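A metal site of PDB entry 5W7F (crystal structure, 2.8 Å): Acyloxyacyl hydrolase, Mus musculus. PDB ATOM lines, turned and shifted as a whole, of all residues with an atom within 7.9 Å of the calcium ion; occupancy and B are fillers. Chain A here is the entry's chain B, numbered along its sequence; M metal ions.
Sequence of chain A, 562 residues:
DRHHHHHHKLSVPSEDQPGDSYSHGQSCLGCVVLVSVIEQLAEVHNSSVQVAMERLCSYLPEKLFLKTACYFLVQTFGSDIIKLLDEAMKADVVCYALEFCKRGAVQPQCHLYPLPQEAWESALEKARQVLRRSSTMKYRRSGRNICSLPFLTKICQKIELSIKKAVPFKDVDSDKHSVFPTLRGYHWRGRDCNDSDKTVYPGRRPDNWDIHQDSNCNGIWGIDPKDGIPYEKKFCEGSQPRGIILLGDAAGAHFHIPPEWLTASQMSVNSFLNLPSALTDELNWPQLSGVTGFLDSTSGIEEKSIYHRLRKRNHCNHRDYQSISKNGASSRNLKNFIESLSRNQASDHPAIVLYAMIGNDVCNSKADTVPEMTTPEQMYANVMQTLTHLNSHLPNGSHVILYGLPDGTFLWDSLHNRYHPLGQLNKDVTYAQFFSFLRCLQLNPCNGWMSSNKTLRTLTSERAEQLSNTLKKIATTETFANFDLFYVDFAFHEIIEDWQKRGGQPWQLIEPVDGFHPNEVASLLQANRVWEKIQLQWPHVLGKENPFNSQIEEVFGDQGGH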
ATOM      1  N   ARG A 204      -3.249  24.741  22.129  1.00  0.00           N
ATOM      2  CA  ARG A 204      -4.240  25.804  22.218  1.00  0.00           C
ATOM      3  C   ARG A 204      -4.329  26.343  23.648  1.00  0.00           C
ATOM      4  O   ARG A 204      -4.166  25.604  24.619  1.00  0.00           O
ATOM      5  CB  ARG A 204      -5.599  25.305  21.742  1.00  0.00           C
ATOM      6  CG  ARG A 204      -6.766  26.211  22.087  1.00  0.00           C
ATOM      7  CD  ARG A 204      -7.867  26.036  21.066  1.00  0.00           C
ATOM      8  NE  ARG A 204      -9.119  26.671  21.463  1.00  0.00           N
ATOM      9  CZ  ARG A 204     -10.056  27.086  20.614  1.00  0.00           C
ATOM     10  NH1 ARG A 204      -9.884  26.947  19.303  1.00  0.00           N
ATOM     11  NH2 ARG A 204     -11.165  27.648  21.078  1.00  0.00           N
ATOM     12  N   ARG A 205      -4.579  27.642  23.753  1.00  0.00           N
ATOM     13  CA  ARG A 205      -4.786  28.254  25.053  1.00  0.00           C
ATOM     14  C   ARG A 205      -6.009  27.627  25.718  1.00  0.00           C
ATOM     15  O   ARG A 205      -6.979  27.274  25.028  1.00  0.00           O
ATOM     16  CB  ARG A 205      -4.958  29.764  24.910  1.00  0.00           C
ATOM     17  CG  ARG A 205      -3.634  30.503  24.722  1.00  0.00           C
ATOM     18  CD  ARG A 205      -3.821  31.994  24.525  1.00  0.00           C
ATOM     19  NE  ARG A 205      -2.546  32.680  24.360  1.00  0.00           N
ATOM     20  CZ  ARG A 205      -2.408  33.991  24.163  1.00  0.00           C
ATOM     21  NH1 ARG A 205      -3.470  34.781  24.108  1.00  0.00           N
ATOM     22  NH2 ARG A 205      -1.198  34.515  24.010  1.00  0.00           N
ATOM     23  N   PRO A 206      -6.009  27.478  27.039  1.00  0.00           N
ATOM     24  CA  PRO A 206      -7.106  26.735  27.690  1.00  0.00           C
ATOM     25  C   PRO A 206      -8.458  27.392  27.454  1.00  0.00           C
ATOM     26  O   PRO A 206      -8.682  28.545  27.814  1.00  0.00           O
ATOM     27  CB  PRO A 206      -6.706  26.768  29.174  1.00  0.00           C
ATOM     28  CG  PRO A 206      -5.861  27.985  29.315  1.00  0.00           C
ATOM     29  CD  PRO A 206      -5.126  28.132  28.023  1.00  0.00           C
ATOM     30  N   ASP A 207      -9.366  26.623  26.838  1.00  0.00           N
ATOM     31  CA  ASP A 207     -10.719  27.076  26.549  1.00  0.00           C
ATOM     32  C   ASP A 207     -11.604  26.819  27.768  1.00  0.00           C
ATOM     33  O   ASP A 207     -11.950  25.671  28.066  1.00  0.00           O
ATOM     34  CB  ASP A 207     -11.282  26.376  25.317  1.00  0.00           C
ATOM     35  CG  ASP A 207     -12.689  26.821  24.980  1.00  0.00           C
ATOM     36  OD1 ASP A 207     -12.846  27.882  24.332  1.00  0.00           O
ATOM     37  OD2 ASP A 207     -13.646  26.108  25.351  1.00  0.00           O
ATOM     38  N   TRP A 209     -10.694  26.669  30.569  1.00  0.00           N
ATOM     39  CA  TRP A 209      -9.926  25.830  31.485  1.00  0.00           C
ATOM     40  C   TRP A 209     -10.609  24.479  31.662  1.00  0.00           C
ATOM     41  O   TRP A 209     -10.632  23.899  32.751  1.00  0.00           O
ATOM     42  CB  TRP A 209      -9.706  26.550  32.807  1.00  0.00           C
ATOM     43  CG  TRP A 209      -8.878  27.787  32.606  1.00  0.00           C
ATOM     44  CD1 TRP A 209      -7.528  27.905  32.748  1.00  0.00           C
ATOM     45  CD2 TRP A 209      -9.351  29.072  32.182  1.00  0.00           C
ATOM     46  NE1 TRP A 209      -7.138  29.183  32.454  1.00  0.00           N
ATOM     47  CE2 TRP A 209      -8.235  29.922  32.104  1.00  0.00           C
ATOM     48  CE3 TRP A 209     -10.614  29.587  31.869  1.00  0.00           C
ATOM     49  CZ2 TRP A 209      -8.341  31.262  31.726  1.00  0.00           C
ATOM     50  CZ3 TRP A 209     -10.719  30.916  31.498  1.00  0.00           C
ATOM     51  CH2 TRP A 209      -9.583  31.731  31.432  1.00  0.00           C
ATOM     52  N   ASP A 210     -11.185  23.998  30.559  1.00  0.00           N
ATOM     53  CA  ASP A 210     -11.701  22.636  30.445  1.00  0.00           C
ATOM     54  C   ASP A 210     -12.665  22.307  31.584  1.00  0.00           C
ATOM     55  O   ASP A 210     -12.486  21.345  32.343  1.00  0.00           O
ATOM     56  CB  ASP A 210     -10.546  21.634  30.368  1.00  0.00           C
ATOM     57  CG  ASP A 210      -9.557  21.972  29.281  1.00  0.00           C
ATOM     58  OD1 ASP A 210      -9.889  22.810  28.415  1.00  0.00           O
ATOM     59  OD2 ASP A 210      -8.442  21.406  29.276  1.00  0.00           O
ATOM     60  N   GLN A 213     -14.716  19.943  28.607  1.00  0.00           N
ATOM     61  CA  GLN A 213     -13.976  19.142  27.649  1.00  0.00           C
ATOM     62  C   GLN A 213     -12.529  19.590  27.607  1.00  0.00           C
ATOM     63  O   GLN A 213     -12.216  20.750  27.908  1.00  0.00           O
ATOM     64  CB  GLN A 213     -14.606  19.246  26.252  1.00  0.00           C
ATOM     65  CG  GLN A 213     -13.926  18.422  25.170  1.00  0.00           C
ATOM     66  CD  GLN A 213     -14.581  18.591  23.809  1.00  0.00           C
ATOM     67  OE1 GLN A 213     -14.772  17.616  23.076  1.00  0.00           O
ATOM     68  NE2 GLN A 213     -14.919  19.824  23.456  1.00  0.00           N
ATOM     69  N   ASP A 214     -11.645  18.670  27.248  1.00  0.00           N
ATOM     70  CA  ASP A 214     -10.232  18.992  27.079  1.00  0.00           C
ATOM     71  C   ASP A 214     -10.055  19.817  25.805  1.00  0.00           C
ATOM     72  O   ASP A 214     -10.349  19.352  24.705  1.00  0.00           O
ATOM     73  CB  ASP A 214      -9.397  17.718  27.009  1.00  0.00           C
ATOM     74  CG  ASP A 214      -7.952  17.940  27.421  1.00  0.00           C
ATOM     75  OD1 ASP A 214      -7.266  16.950  27.749  1.00  0.00           O
ATOM     76  OD2 ASP A 214      -7.511  19.112  27.429  1.00  0.00           O
ATOM     77  N   SER A 215      -9.560  21.047  25.964  1.00  0.00           N
ATOM     78  CA  SER A 215      -9.459  21.968  24.838  1.00  0.00           C
ATOM     79  C   SER A 215      -8.196  21.736  24.022  1.00  0.00           C
ATOM     80  O   SER A 215      -8.221  21.847  22.788  1.00  0.00           O
ATOM     81  CB  SER A 215      -9.512  23.402  25.336  1.00  0.00           C
ATOM     82  OG  SER A 215      -8.429  23.679  26.216  1.00  0.00           O
ATOM     83  N   ASN A 216      -7.080  21.422  24.685  1.00  0.00           N
ATOM     84  CA  ASN A 216      -5.793  21.247  24.032  1.00  0.00           C
ATOM     85  C   ASN A 216      -5.282  19.814  24.116  1.00  0.00           C
ATOM     86  O   ASN A 216      -4.072  19.578  24.030  1.00  0.00           O
ATOM     87  CB  ASN A 216      -4.770  22.220  24.622  1.00  0.00           C
ATOM     88  CG  ASN A 216      -4.828  22.290  26.136  1.00  0.00           C
ATOM     89  OD1 ASN A 216      -5.309  21.363  26.787  1.00  0.00           O
ATOM     90  ND2 ASN A 216      -4.356  23.400  26.692  1.00  0.00           N
ATOM     91  N   CYS A 217      -6.184  18.843  24.286  1.00  0.00           N
ATOM     92  CA  CYS A 217      -5.828  17.422  24.302  1.00  0.00           C
ATOM     93  C   CYS A 217      -4.631  17.136  25.210  1.00  0.00           C
ATOM     94  O   CYS A 217      -3.946  16.125  25.041  1.00  0.00           O
ATOM     95  CB  CYS A 217      -5.546  16.910  22.894  1.00  0.00           C
ATOM     96  SG  CYS A 217      -6.919  17.057  21.714  1.00  0.00           S
ATOM     97  N   ASN A 218      -4.355  18.006  26.181  1.00  0.00           N
ATOM     98  CA  ASN A 218      -3.235  17.817  27.084  1.00  0.00           C
ATOM     99  C   ASN A 218      -3.608  16.973  28.297  1.00  0.00           C
ATOM    100  O   ASN A 218      -2.832  16.901  29.260  1.00  0.00           O
ATOM    101  CB  ASN A 218      -2.692  19.177  27.543  1.00  0.00           C
ATOM    102  CG  ASN A 218      -3.431  19.733  28.748  1.00  0.00           C
ATOM    103  OD1 ASN A 218      -4.650  19.574  28.874  1.00  0.00           O
ATOM    104  ND2 ASN A 218      -2.696  20.395  29.631  1.00  0.00           N
ATOM    105  N   GLY A 219      -4.776  16.320  28.276  1.00  0.00           N
ATOM    106  CA  GLY A 219      -5.147  15.371  29.303  1.00  0.00           C
ATOM    107  C   GLY A 219      -5.688  15.973  30.584  1.00  0.00           C
ATOM    108  O   GLY A 219      -5.969  15.220  31.533  1.00  0.00           O
ATOM    109  N   ILE A 220      -5.859  17.295  30.658  1.00  0.00           N
ATOM    110  CA  ILE A 220      -6.322  17.970  31.867  1.00  0.00           C
ATOM    111  C   ILE A 220      -7.690  18.564  31.588  1.00  0.00           C
ATOM    112  O   ILE A 220      -7.860  19.341  30.636  1.00  0.00           O
ATOM    113  CB  ILE A 220      -5.327  19.042  32.325  1.00  0.00           C
ATOM    114  CG1 ILE A 220      -3.986  18.395  32.667  1.00  0.00           C
ATOM    115  CG2 ILE A 220      -5.889  19.816  33.521  1.00  0.00           C
ATOM    116  CD1 ILE A 220      -2.913  19.371  33.130  1.00  0.00           C
ATOM    117  N   TRP A 221      -8.670  18.208  32.415  1.00  0.00           N
ATOM    118  CA  TRP A 221     -10.014  18.764  32.321  1.00  0.00           C
ATOM    119  C   TRP A 221     -10.718  18.547  33.648  1.00  0.00           C
ATOM    120  O   TRP A 221     -10.229  17.849  34.542  1.00  0.00           O
ATOM    121  CB  TRP A 221     -10.818  18.128  31.181  1.00  0.00           C
ATOM    122  CG  TRP A 221     -11.138  16.686  31.416  1.00  0.00           C
ATOM    123  CD1 TRP A 221     -10.367  15.610  31.094  1.00  0.00           C
ATOM    124  CD2 TRP A 221     -12.309  16.160  32.067  1.00  0.00           C
ATOM    125  NE1 TRP A 221     -10.997  14.448  31.481  1.00  0.00           N
ATOM    126  CE2 TRP A 221     -12.183  14.761  32.083  1.00  0.00           C
ATOM    127  CE3 TRP A 221     -13.449  16.745  32.630  1.00  0.00           C
ATOM    128  CZ2 TRP A 221     -13.150  13.927  32.645  1.00  0.00           C
ATOM    129  CZ3 TRP A 221     -14.406  15.923  33.183  1.00  0.00           C
ATOM    130  CH2 TRP A 221     -14.251  14.524  33.188  1.00  0.00           C
ATOM    131  N   GLY A 222     -11.893  19.163  33.770  1.00  0.00           N
ATOM    132  CA  GLY A 222     -12.706  19.031  34.958  1.00  0.00           C
ATOM    133  C   GLY A 222     -12.469  20.142  35.962  1.00  0.00           C
ATOM    134  O   GLY A 222     -11.835  21.158  35.687  1.00  0.00           O
ATOM    135  N   TYR A 231      -9.284  22.290  37.377  1.00  0.00           N
ATOM    136  CA  TYR A 231      -7.978  21.665  37.520  1.00  0.00           C
ATOM    137  C   TYR A 231      -6.917  22.375  36.690  1.00  0.00           C
ATOM    138  O   TYR A 231      -5.781  22.554  37.137  1.00  0.00           O
ATOM    139  CB  TYR A 231      -8.048  20.195  37.127  1.00  0.00           C
ATOM    140  CG  TYR A 231      -8.322  19.219  38.264  1.00  0.00           C
ATOM    141  CD1 TYR A 231      -9.261  18.204  38.110  1.00  0.00           C
ATOM    142  CD2 TYR A 231      -7.632  19.298  39.459  1.00  0.00           C
ATOM    143  CE1 TYR A 231      -9.510  17.310  39.139  1.00  0.00           C
ATOM    144  CE2 TYR A 231      -7.871  18.403  40.488  1.00  0.00           C
ATOM    145  CZ  TYR A 231      -8.810  17.412  40.318  1.00  0.00           C
ATOM    146  OH  TYR A 231      -9.059  16.528  41.350  1.00  0.00           O
ATOM    147  N   GLU A 232      -7.280  22.794  35.483  1.00  0.00           N
ATOM    148  CA  GLU A 232      -6.311  23.367  34.549  1.00  0.00           C
ATOM    149  C   GLU A 232      -5.631  24.603  35.137  1.00  0.00           C
ATOM    150  O   GLU A 232      -4.418  24.574  35.381  1.00  0.00           O
ATOM    151  CB  GLU A 232      -6.996  23.732  33.231  1.00  0.00           C
ATOM    152  CG  GLU A 232      -6.053  24.217  32.137  1.00  0.00           C
ATOM    153  CD  GLU A 232      -5.356  23.073  31.418  1.00  0.00           C
ATOM    154  OE1 GLU A 232      -5.989  22.022  31.213  1.00  0.00           O
ATOM    155  OE2 GLU A 232      -4.176  23.235  31.038  1.00  0.00           O
ATOM    156  N   LYS A 233      -6.390  25.675  35.374  1.00  0.00           N
ATOM    157  CA  LYS A 233      -5.764  26.931  35.776  1.00  0.00           C
ATOM    158  C   LYS A 233      -5.003  26.779  37.081  1.00  0.00           C
ATOM    159  O   LYS A 233      -3.856  27.210  37.191  1.00  0.00           O
ATOM    160  CB  LYS A 233      -6.822  28.031  35.898  1.00  0.00           C
ATOM    161  CG  LYS A 233      -6.245  29.390  35.515  1.00  0.00           C
ATOM    162  CD  LYS A 233      -7.280  30.492  35.421  1.00  0.00           C
ATOM    163  CE  LYS A 233      -6.671  31.764  34.853  1.00  0.00           C
ATOM    164  NZ  LYS A 233      -5.196  31.865  35.054  1.00  0.00           N
ATOM    165  N   CYS A 236      -1.978  24.879  35.646  1.00  0.00           N
ATOM    166  CA  CYS A 236      -1.202  25.322  34.494  1.00  0.00           C
ATOM    167  C   CYS A 236      -1.026  26.838  34.439  1.00  0.00           C
ATOM    168  O   CYS A 236      -0.177  27.321  33.670  1.00  0.00           O
ATOM    169  CB  CYS A 236      -1.853  24.855  33.194  1.00  0.00           C
ATOM    170  SG  CYS A 236      -1.753  23.065  32.926  1.00  0.00           S
ATOM    171  N   CYS A 316       1.837  20.438  31.462  1.00  0.00           N
ATOM    172  CA  CYS A 316       0.857  21.082  30.602  1.00  0.00           C
ATOM    173  C   CYS A 316       1.292  21.054  29.141  1.00  0.00           C
ATOM    174  O   CYS A 316       0.447  21.024  28.244  1.00  0.00           O
ATOM    175  CB  CYS A 316       0.619  22.524  31.054  1.00  0.00           C
ATOM    176  SG  CYS A 316       0.243  22.671  32.822  1.00  0.00           S
ATOM    177  N   HIS A 349      -0.527  28.920  22.671  1.00  0.00           N
ATOM    178  CA  HIS A 349       0.551  29.295  23.572  1.00  0.00           C
ATOM    179  C   HIS A 349       1.784  29.698  22.758  1.00  0.00           C
ATOM    180  O   HIS A 349       1.822  29.536  21.543  1.00  0.00           O
ATOM    181  CB  HIS A 349       0.906  28.129  24.491  1.00  0.00           C
ATOM    182  CG  HIS A 349      -0.221  27.704  25.386  1.00  0.00           C
ATOM    183  ND1 HIS A 349      -0.476  28.295  26.603  1.00  0.00           N
ATOM    184  CD2 HIS A 349      -1.149  26.728  25.239  1.00  0.00           C
ATOM    185  CE1 HIS A 349      -1.515  27.709  27.170  1.00  0.00           C
ATOM    186  NE2 HIS A 349      -1.942  26.750  26.366  1.00  0.00           N
HETATM  187 CA    CA M   1      -6.154  21.531  28.962  1.00  0.00          CA
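OD2 of Asp 210 sits close to O of Ile 220, at 2.5 Å.
The backbone NH (N) of Gly 222 sits at hydrogen-bond distance from the backbone carbonyl oxygen (O) of Asp 210.
The side-chain carboxylate of Asp 214 is in hydrogen-bond range of the backbone NH of Cys 217 (3.4 Å).
The side-chain carboxylate (OD1) of Asp 210 lies within hydrogen-bond range of the side-chain hydroxyl (OG) of Ser 215 (2.8 Å).
SG of Cys 236 is disulfide-bonded to SG of Cys 316 (2.0 Å).
OD1 of Asn 218 sits close to N of Ile 220 (3.1 Å).
O of Arg 204 sits at hydrogen-bond distance from ND2 of Asn 216 (3.0 Å).
The side-chain amide oxygen (OD1) of Asn 216 lies close to the side-chain carboxylate (OD2) of Asp 214 (3.2 Å).
Residues that only touch the calcium ion: Asp 214 and Ile 220.
Within 4 Å of the calcium ion: Asp 210, Asp 214, Asn 216, Asn 218, Ile 220 and Glu 232.
The nearest printed residue that does not touch the calcium ion is Ser 215 (4.2 Å).
The calcium ion is bound by OE1 of Glu 232 (2.3 Å), OD2 of Asp 210 (2.3 Å), OD1 of Asn 216 (2.3 Å) and OD1 of Asn 218 (2.5 Å).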
